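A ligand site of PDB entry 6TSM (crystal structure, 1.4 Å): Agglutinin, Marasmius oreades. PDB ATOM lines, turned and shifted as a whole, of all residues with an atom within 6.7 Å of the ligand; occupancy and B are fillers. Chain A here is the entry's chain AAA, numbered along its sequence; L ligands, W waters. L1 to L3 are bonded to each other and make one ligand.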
ATOM      1  N   HIS A   9     -25.019 -17.765  -7.383  1.00  0.00           N
ATOM      2  CA  HIS A   9     -24.532 -16.608  -8.147  1.00  0.00           C
ATOM      3  C   HIS A   9     -23.846 -15.640  -7.189  1.00  0.00           C
ATOM      4  O   HIS A   9     -24.491 -15.240  -6.233  1.00  0.00           O
ATOM      5  CB  HIS A   9     -25.690 -15.947  -8.867  1.00  0.00           C
ATOM      6  CG  HIS A   9     -25.289 -14.964  -9.921  1.00  0.00           C
ATOM      7  ND1 HIS A   9     -25.563 -13.607  -9.822  1.00  0.00           N
ATOM      8  CD2 HIS A   9     -24.559 -15.114 -11.052  1.00  0.00           C
ATOM      9  CE1 HIS A   9     -25.065 -12.982 -10.872  1.00  0.00           C
ATOM     10  NE2 HIS A   9     -24.469 -13.876 -11.647  1.00  0.00           N
ATOM     11  N   ASP A  20     -17.055 -14.725 -12.434  1.00  0.00           N
ATOM     12  CA  ASP A  20     -17.297 -15.198 -13.801  1.00  0.00           C
ATOM     13  C   ASP A  20     -16.094 -16.026 -14.240  1.00  0.00           C
ATOM     14  O   ASP A  20     -14.968 -15.528 -14.130  1.00  0.00           O
ATOM     15  CB  ASP A  20     -17.572 -14.018 -14.736  1.00  0.00           C
ATOM     16  CG  ASP A  20     -17.929 -14.377 -16.164  1.00  0.00           C
ATOM     17  OD1 ASP A  20     -17.073 -14.938 -16.828  1.00  0.00           O
ATOM     18  OD2 ASP A  20     -19.039 -13.952 -16.627  1.00  0.00           O
ATOM     19  N   LEU A  21     -16.315 -17.242 -14.676  1.00  0.00           N
ATOM     20  CA  LEU A  21     -15.236 -18.011 -15.345  1.00  0.00           C
ATOM     21  C   LEU A  21     -15.156 -17.570 -16.797  1.00  0.00           C
ATOM     22  O   LEU A  21     -16.129 -17.853 -17.566  1.00  0.00           O
ATOM     23  CB  LEU A  21     -15.537 -19.507 -15.253  1.00  0.00           C
ATOM     24  CG  LEU A  21     -14.476 -20.435 -15.884  1.00  0.00           C
ATOM     25  CD1 LEU A  21     -13.136 -20.281 -15.210  1.00  0.00           C
ATOM     26  CD2 LEU A  21     -14.930 -21.883 -15.833  1.00  0.00           C
ATOM     27  N   LYS A  22     -14.053 -16.938 -17.192  1.00  0.00           N
ATOM     28  CA  LYS A  22     -14.018 -16.178 -18.460  1.00  0.00           C
ATOM     29  C   LYS A  22     -14.328 -17.136 -19.643  1.00  0.00           C
ATOM     30  O   LYS A  22     -13.622 -18.167 -19.800  1.00  0.00           O
ATOM     31  CB  LYS A  22     -12.681 -15.471 -18.658  1.00  0.00           C
ATOM     32  CG  LYS A  22     -12.747 -14.295 -19.593  1.00  0.00           C
ATOM     33  CD  LYS A  22     -11.503 -13.467 -19.676  1.00  0.00           C
ATOM     34  CE  LYS A  22     -11.650 -12.329 -20.673  1.00  0.00           C
ATOM     35  NZ  LYS A  22     -10.537 -11.344 -20.559  1.00  0.00           N
ATOM     36  N   ASP A  23     -15.322 -16.757 -20.453  1.00  0.00           N
ATOM     37  CA  ASP A  23     -15.782 -17.488 -21.668  1.00  0.00           C
ATOM     38  C   ASP A  23     -16.262 -18.913 -21.289  1.00  0.00           C
ATOM     39  O   ASP A  23     -16.487 -19.708 -22.208  1.00  0.00           O
ATOM     40  CB  ASP A  23     -14.683 -17.545 -22.713  1.00  0.00           C
ATOM     41  CG  ASP A  23     -15.223 -17.686 -24.125  1.00  0.00           C
ATOM     42  OD1 ASP A  23     -16.319 -17.164 -24.391  1.00  0.00           O
ATOM     43  OD2 ASP A  23     -14.590 -18.417 -24.915  1.00  0.00           O
ATOM     44  N   GLY A  24     -16.439 -19.188 -20.011  1.00  0.00           N
ATOM     45  CA  GLY A  24     -16.877 -20.507 -19.546  1.00  0.00           C
ATOM     46  C   GLY A  24     -15.843 -21.605 -19.858  1.00  0.00           C
ATOM     47  O   GLY A  24     -16.219 -22.771 -19.895  1.00  0.00           O
ATOM     48  N   VAL A  33     -12.956 -13.797 -13.139  1.00  0.00           N
ATOM     49  CA  VAL A  33     -12.957 -12.327 -13.275  1.00  0.00           C
ATOM     50  C   VAL A  33     -14.310 -11.785 -12.763  1.00  0.00           C
ATOM     51  O   VAL A  33     -15.291 -12.541 -12.734  1.00  0.00           O
ATOM     52  CB  VAL A  33     -12.713 -11.904 -14.730  1.00  0.00           C
ATOM     53  CG1 VAL A  33     -11.327 -12.307 -15.209  1.00  0.00           C
ATOM     54  CG2 VAL A  33     -13.781 -12.447 -15.667  1.00  0.00           C
ATOM     55  N   TRP A  35     -17.601  -9.632 -13.614  1.00  0.00           N
ATOM     56  CA  TRP A  35     -18.366  -9.378 -14.864  1.00  0.00           C
ATOM     57  C   TRP A  35     -19.776  -8.959 -14.508  1.00  0.00           C
ATOM     58  O   TRP A  35     -20.343  -9.517 -13.567  1.00  0.00           O
ATOM     59  CB  TRP A  35     -18.355 -10.640 -15.774  1.00  0.00           C
ATOM     60  CG  TRP A  35     -18.516 -10.340 -17.227  1.00  0.00           C
ATOM     61  CD1 TRP A  35     -19.658  -9.997 -17.879  1.00  0.00           C
ATOM     62  CD2 TRP A  35     -17.468 -10.315 -18.216  1.00  0.00           C
ATOM     63  NE1 TRP A  35     -19.394  -9.769 -19.218  1.00  0.00           N
ATOM     64  CE2 TRP A  35     -18.057  -9.936 -19.446  1.00  0.00           C
ATOM     65  CE3 TRP A  35     -16.078 -10.533 -18.166  1.00  0.00           C
ATOM     66  CZ2 TRP A  35     -17.300  -9.777 -20.602  1.00  0.00           C
ATOM     67  CZ3 TRP A  35     -15.339 -10.395 -19.314  1.00  0.00           C
ATOM     68  CH2 TRP A  35     -15.944 -10.010 -20.516  1.00  0.00           C
ATOM     69  N   GLN A  36     -20.371  -8.119 -15.298  1.00  0.00           N
ATOM     70  CA  GLN A  36     -21.762  -7.681 -15.043  1.00  0.00           C
ATOM     71  C   GLN A  36     -22.734  -8.834 -15.366  1.00  0.00           C
ATOM     72  O   GLN A  36     -22.326  -9.807 -16.027  1.00  0.00           O
ATOM     73  CB  GLN A  36     -22.105  -6.424 -15.874  1.00  0.00           C
ATOM     74  CG  GLN A  36     -22.133  -6.631 -17.358  1.00  0.00           C
ATOM     75  CD  GLN A  36     -22.528  -5.371 -18.100  1.00  0.00           C
ATOM     76  OE1 GLN A  36     -23.622  -4.840 -17.922  1.00  0.00           O
ATOM     77  NE2 GLN A  36     -21.599  -4.833 -18.853  1.00  0.00           N
ATOM     78  N   PHE A  37     -23.968  -8.709 -14.925  1.00  0.00           N
ATOM     79  CA  PHE A  37     -24.919  -9.822 -14.995  1.00  0.00           C
ATOM     80  C   PHE A  37     -26.323  -9.273 -15.212  1.00  0.00           C
ATOM     81  O   PHE A  37     -26.533  -8.072 -15.090  1.00  0.00           O
ATOM     82  CB  PHE A  37     -24.821 -10.676 -13.721  1.00  0.00           C
ATOM     83  CG  PHE A  37     -25.054  -9.927 -12.433  1.00  0.00           C
ATOM     84  CD1 PHE A  37     -26.332  -9.820 -11.892  1.00  0.00           C
ATOM     85  CD2 PHE A  37     -23.992  -9.418 -11.705  1.00  0.00           C
ATOM     86  CE1 PHE A  37     -26.530  -9.169 -10.685  1.00  0.00           C
ATOM     87  CE2 PHE A  37     -24.206  -8.772 -10.496  1.00  0.00           C
ATOM     88  CZ  PHE A  37     -25.467  -8.655  -9.990  1.00  0.00           C
ATOM     89  N   THR A  38     -27.199 -10.126 -15.678  1.00  0.00           N
ATOM     90  CA  THR A  38     -28.625  -9.782 -15.861  1.00  0.00           C
ATOM     91  C   THR A  38     -29.453 -10.596 -14.870  1.00  0.00           C
ATOM     92  O   THR A  38     -29.505 -11.806 -14.964  1.00  0.00           O
ATOM     93  CB  THR A  38     -29.075 -10.025 -17.303  1.00  0.00           C
ATOM     94  OG1 THR A  38     -28.093  -9.431 -18.186  1.00  0.00           O
ATOM     95  CG2 THR A  38     -30.444  -9.457 -17.589  1.00  0.00           C
ATOM     96  N   PRO A  39     -30.121  -9.950 -13.913  1.00  0.00           N
ATOM     97  CA  PRO A  39     -31.008 -10.677 -12.985  1.00  0.00           C
ATOM     98  C   PRO A  39     -32.144 -11.400 -13.730  1.00  0.00           C
ATOM     99  O   PRO A  39     -32.541 -10.927 -14.779  1.00  0.00           O
ATOM    100  CB  PRO A  39     -31.590  -9.567 -12.072  1.00  0.00           C
ATOM    101  CG  PRO A  39     -30.627  -8.371 -12.260  1.00  0.00           C
ATOM    102  CD  PRO A  39     -30.101  -8.515 -13.678  1.00  0.00           C
ATOM    103  N   THR A  41     -32.144 -14.161 -15.317  1.00  0.00           N
ATOM    104  CA  THR A  41     -31.685 -14.986 -16.419  1.00  0.00           C
ATOM    105  C   THR A  41     -30.838 -16.121 -15.865  1.00  0.00           C
ATOM    106  O   THR A  41     -30.393 -16.008 -14.683  1.00  0.00           O
ATOM    107  CB  THR A  41     -30.864 -14.183 -17.452  1.00  0.00           C
ATOM    108  OG1 THR A  41     -29.594 -13.817 -16.856  1.00  0.00           O
ATOM    109  CG2 THR A  41     -31.569 -12.954 -17.943  1.00  0.00           C
ATOM    110  N   ILE A  42     -30.481 -17.055 -16.714  1.00  0.00           N
ATOM    111  CA  ILE A  42     -29.303 -17.926 -16.495  1.00  0.00           C
ATOM    112  C   ILE A  42     -28.049 -17.147 -16.911  1.00  0.00           C
ATOM    113  O   ILE A  42     -27.940 -16.790 -18.118  1.00  0.00           O
ATOM    114  CB  ILE A  42     -29.441 -19.235 -17.274  1.00  0.00           C
ATOM    115  CG1 ILE A  42     -30.649 -20.060 -16.790  1.00  0.00           C
ATOM    116  CG2 ILE A  42     -28.164 -20.032 -17.215  1.00  0.00           C
ATOM    117  CD1 ILE A  42     -30.586 -20.440 -15.352  1.00  0.00           C
ATOM    118  N   ASN A  43     -27.216 -16.792 -15.938  1.00  0.00           N
ATOM    119  CA  ASN A  43     -25.898 -16.201 -16.201  1.00  0.00           C
ATOM    120  C   ASN A  43     -24.880 -17.342 -16.395  1.00  0.00           C
ATOM    121  O   ASN A  43     -24.376 -17.890 -15.372  1.00  0.00           O
ATOM    122  CB  ASN A  43     -25.490 -15.210 -15.100  1.00  0.00           C
ATOM    123  CG  ASN A  43     -26.353 -13.958 -15.120  1.00  0.00           C
ATOM    124  OD1 ASN A  43     -26.148 -13.080 -15.933  1.00  0.00           O
ATOM    125  ND2 ASN A  43     -27.345 -13.891 -14.238  1.00  0.00           N
ATOM    126  N   TRP A  44     -24.688 -17.759 -17.642  1.00  0.00           N
ATOM    127  CA  TRP A  44     -24.160 -19.084 -18.009  1.00  0.00           C
ATOM    128  C   TRP A  44     -22.788 -19.333 -17.375  1.00  0.00           C
ATOM    129  O   TRP A  44     -22.467 -20.511 -17.134  1.00  0.00           O
ATOM    130  CB  TRP A  44     -24.100 -19.199 -19.538  1.00  0.00           C
ATOM    131  CG  TRP A  44     -25.402 -19.528 -20.150  1.00  0.00           C
ATOM    132  CD1 TRP A  44     -26.350 -18.663 -20.637  1.00  0.00           C
ATOM    133  CD2 TRP A  44     -26.004 -20.824 -20.177  1.00  0.00           C
ATOM    134  NE1 TRP A  44     -27.453 -19.349 -21.020  1.00  0.00           N
ATOM    135  CE2 TRP A  44     -27.280 -20.681 -20.747  1.00  0.00           C
ATOM    136  CE3 TRP A  44     -25.590 -22.079 -19.761  1.00  0.00           C
ATOM    137  CZ2 TRP A  44     -28.116 -21.769 -20.971  1.00  0.00           C
ATOM    138  CZ3 TRP A  44     -26.418 -23.157 -19.989  1.00  0.00           C
ATOM    139  CH2 TRP A  44     -27.669 -22.998 -20.565  1.00  0.00           C
ATOM    140  N   HIS A  45     -21.941 -18.301 -17.265  1.00  0.00           N
ATOM    141  CA  HIS A  45     -20.519 -18.519 -16.806  1.00  0.00           C
ATOM    142  C   HIS A  45     -20.355 -18.150 -15.334  1.00  0.00           C
ATOM    143  O   HIS A  45     -19.206 -18.192 -14.858  1.00  0.00           O
ATOM    144  CB  HIS A  45     -19.548 -17.735 -17.687  1.00  0.00           C
ATOM    145  CG  HIS A  45     -19.683 -18.031 -19.135  1.00  0.00           C
ATOM    146  ND1 HIS A  45     -19.273 -17.145 -20.108  1.00  0.00           N
ATOM    147  CD2 HIS A  45     -20.093 -19.149 -19.788  1.00  0.00           C
ATOM    148  CE1 HIS A  45     -19.499 -17.665 -21.307  1.00  0.00           C
ATOM    149  NE2 HIS A  45     -20.000 -18.873 -21.154  1.00  0.00           N
ATOM    150  N   GLN A  46     -21.455 -17.947 -14.606  1.00  0.00           N
ATOM    151  CA  GLN A  46     -21.416 -17.270 -13.272  1.00  0.00           C
ATOM    152  C   GLN A  46     -22.168 -18.098 -12.235  1.00  0.00           C
ATOM    153  O   GLN A  46     -22.500 -17.540 -11.191  1.00  0.00           O
ATOM    154  CB  GLN A  46     -22.027 -15.879 -13.368  1.00  0.00           C
ATOM    155  CG  GLN A  46     -21.337 -14.990 -14.395  1.00  0.00           C
ATOM    156  CD  GLN A  46     -21.952 -13.606 -14.496  1.00  0.00           C
ATOM    157  OE1 GLN A  46     -23.003 -13.307 -13.878  1.00  0.00           O
ATOM    158  NE2 GLN A  46     -21.342 -12.755 -15.309  1.00  0.00           N
ATOM    159  N   PHE A  66     -21.065 -24.578 -15.610  1.00  0.00           N
ATOM    160  CA  PHE A  66     -20.946 -24.684 -17.071  1.00  0.00           C
ATOM    161  C   PHE A  66     -19.693 -25.514 -17.439  1.00  0.00           C
ATOM    162  O   PHE A  66     -19.832 -26.451 -18.216  1.00  0.00           O
ATOM    163  CB  PHE A  66     -20.890 -23.288 -17.697  1.00  0.00           C
ATOM    164  CG  PHE A  66     -20.831 -23.279 -19.202  1.00  0.00           C
ATOM    165  CD1 PHE A  66     -21.972 -23.457 -19.968  1.00  0.00           C
ATOM    166  CD2 PHE A  66     -19.621 -23.152 -19.861  1.00  0.00           C
ATOM    167  CE1 PHE A  66     -21.899 -23.445 -21.350  1.00  0.00           C
ATOM    168  CE2 PHE A  66     -19.561 -23.181 -21.250  1.00  0.00           C
ATOM    169  CZ  PHE A  66     -20.702 -23.289 -21.984  1.00  0.00           C
ATOM    170  N   ASP A 131     -15.896  -5.188 -16.882  1.00  0.00           N
ATOM    171  CA  ASP A 131     -16.035  -6.592 -17.342  1.00  0.00           C
ATOM    172  C   ASP A 131     -14.642  -7.172 -17.590  1.00  0.00           C
ATOM    173  O   ASP A 131     -13.882  -6.602 -18.408  1.00  0.00           O
ATOM    174  CB  ASP A 131     -16.887  -6.693 -18.587  1.00  0.00           C
ATOM    175  CG  ASP A 131     -18.347  -6.386 -18.347  1.00  0.00           C
ATOM    176  OD1 ASP A 131     -18.776  -6.456 -17.173  1.00  0.00           O
ATOM    177  OD2 ASP A 131     -19.014  -5.993 -19.300  1.00  0.00           O
HETATM  178  C1  LIG L   1     -23.483 -14.012 -22.473  1.00  0.00           C
HETATM  179  C2  LIG L   1     -24.297 -13.500 -23.651  1.00  0.00           C
HETATM  180  C3  LIG L   1     -23.988 -14.290 -24.912  1.00  0.00           C
HETATM  181  C4  LIG L   1     -24.110 -15.775 -24.658  1.00  0.00           C
HETATM  182  C5  LIG L   1     -23.246 -16.192 -23.473  1.00  0.00           C
HETATM  183  C6  LIG L   1     -23.369 -17.639 -23.174  1.00  0.00           C
HETATM  184  O1  LIG L   1     -24.002 -12.124 -23.861  1.00  0.00           O
HETATM  185  O2  LIG L   1     -24.891 -13.884 -25.992  1.00  0.00           O
HETATM  186  O3  LIG L   1     -25.488 -16.139 -24.394  1.00  0.00           O
HETATM  187  O4  LIG L   1     -23.667 -15.446 -22.305  1.00  0.00           O
HETATM  188  C1  LG2 L   2     -19.914 -14.209 -22.484  1.00  0.00           C
HETATM  189  C2  LG2 L   2     -21.224 -14.066 -21.729  1.00  0.00           C
HETATM  190  C3  LG2 L   2     -21.123 -13.034 -20.631  1.00  0.00           C
HETATM  191  C4  LG2 L   2     -19.914 -13.276 -19.743  1.00  0.00           C
HETATM  192  C5  LG2 L   2     -18.657 -13.417 -20.639  1.00  0.00           C
HETATM  193  C6  LG2 L   2     -17.356 -13.656 -19.842  1.00  0.00           C
HETATM  194  O1  LG2 L   2     -20.008 -15.290 -23.314  1.00  0.00           O
HETATM  195  O2  LG2 L   2     -22.229 -13.679 -22.681  1.00  0.00           O
HETATM  196  O3  LG2 L   2     -22.368 -13.035 -19.873  1.00  0.00           O
HETATM  197  O4  LG2 L   2     -20.097 -14.459 -18.936  1.00  0.00           O
HETATM  198  O5  LG2 L   2     -18.850 -14.485 -21.562  1.00  0.00           O
HETATM  199  O6  LG2 L   2     -17.270 -15.006 -19.410  1.00  0.00           O
HETATM  200  C1  LG3 L   3     -22.523 -12.090 -18.930  1.00  0.00           C
HETATM  201  C2  LG3 L   3     -23.909 -12.116 -18.250  1.00  0.00           C
HETATM  202  C3  LG3 L   3     -24.959 -11.550 -19.197  1.00  0.00           C
HETATM  203  C4  LG3 L   3     -24.504 -10.178 -19.685  1.00  0.00           C
HETATM  204  C5  LG3 L   3     -23.140 -10.324 -20.344  1.00  0.00           C
HETATM  205  C6  LG3 L   3     -22.610  -9.018 -20.894  1.00  0.00           C
HETATM  206  O1  LG3 L   3     -24.258 -13.430 -17.900  1.00  0.00           O
HETATM  207  O2  LG3 L   3     -26.201 -11.457 -18.526  1.00  0.00           O
HETATM  208  O3  LG3 L   3     -24.439  -9.250 -18.612  1.00  0.00           O
HETATM  209  O4  LG3 L   3     -22.234 -10.785 -19.348  1.00  0.00           O
HETATM  210  O5  LG3 L   3     -21.332  -9.221 -21.555  1.00  0.00           O
HETATM  211  O   HOH W   1     -21.497 -10.801 -23.836  1.00  0.00           O
HETATM  212  O   HOH W   2     -25.361 -15.494 -19.636  1.00  0.00           O
HETATM  213  O   HOH W   3     -22.355 -15.538 -17.818  1.00  0.00           O
HETATM  214  O   HOH W   4     -19.532  -7.216 -21.830  1.00  0.00           O
HETATM  215  O   HOH W   5     -26.905 -15.340 -22.084  1.00  0.00           O
HETATM  216  O   HOH W   6     -25.060 -15.806 -27.956  1.00  0.00           O
HETATM  217  O   HOH W   7     -25.840 -10.446 -22.691  1.00  0.00           O
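O of His 45 sits at hydrogen-bond distance from N of Leu 21, at 3.0 Å.
ND2 of Asn 43 sits at hydrogen-bond distance from O of Thr 38 (3.1 Å).
OG1 of Thr 41 sits at hydrogen-bond distance from ND2 of Asn 43.
The side-chain carboxylate (OD2) of Asp 20 is in hydrogen-bond range of the side-chain amide nitrogen (NE2) of Gln 46 (2.9 Å).
The backbone carbonyl oxygen of Gln 36 sits at hydrogen-bond distance from the side-chain amide nitrogen of Gln 46 (3.2 Å).
O of Thr 38 is in hydrogen-bond range of OG1 of Thr 41, 2.8 Å away.
OE1 of Gln 46 is in hydrogen-bond range of NE2 of His 9 (2.7 Å).
The backbone carbonyl oxygen of Val 33 sits at hydrogen-bond distance from the backbone NH of Asp 20 (2.8 Å).
O2 of LG3 L3 lies within hydrogen-bond range of OG1 of Thr 38 (2.8 Å).
OD1 of Asn 43 sits at hydrogen-bond distance from O1 of LG3 L3 (2.8 Å).
The backbone NH (N) of Thr 38 sits at hydrogen-bond distance from an oxygen (O2) of LG3 L3 (3.3 Å).
An oxygen (O4) of LG2 L2 is in hydrogen-bond range of the side-chain carboxylate of Asp 20 (2.6 Å).
An oxygen (O4) of LG3 L3 lies within hydrogen-bond range of the indole nitrogen of Trp 35 (3.0 Å).
N of Asp 23 is in hydrogen-bond range of O6 of LG2 L2, at 2.8 Å.
The backbone carbonyl oxygen (O) of Gln 36 is in hydrogen-bond range of an oxygen (O3) of LG3 L3.
A ring nitrogen (ND1) of His 45 lies within hydrogen-bond range of an oxygen (O6) of LG2 L2, at 3.0 Å.
Water W4 bridges an oxygen (O5) of LG3 L3 and the side-chain carboxylate of Asp 131.
Water W3 lies within hydrogen-bond range of O4 of LG2 L2 (2.7 Å), N of His 45 (2.8 Å) and N of Trp 44 (3.2 Å).
Water W2 lies within hydrogen-bond range of O1 of LG3 L3 (2.9 Å), N of Trp 44 (3.1 Å) and O of Ile 42 (3.3 Å).
Leu 21 touches the ligand.
CA of Lys 22 touches O6 of LG2 L2, 3.6 Å away.
CA of Phe 37 touches O3 of LG3 L3 (3.7 Å).
Gln 46 touches the ligand.
Within 4 Å of the ligand: Asp 20, Leu 21, Lys 22, Asp 23, Trp 35, Gln 36, Phe 37, Thr 38, Asn 43, His 45 and Gln 46.
Along chain A the residues within 4 Å of the ligand span positions 20 to 46.
The nearest printed residue that does not touch the ligand is Trp 44 (4.02 Å).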
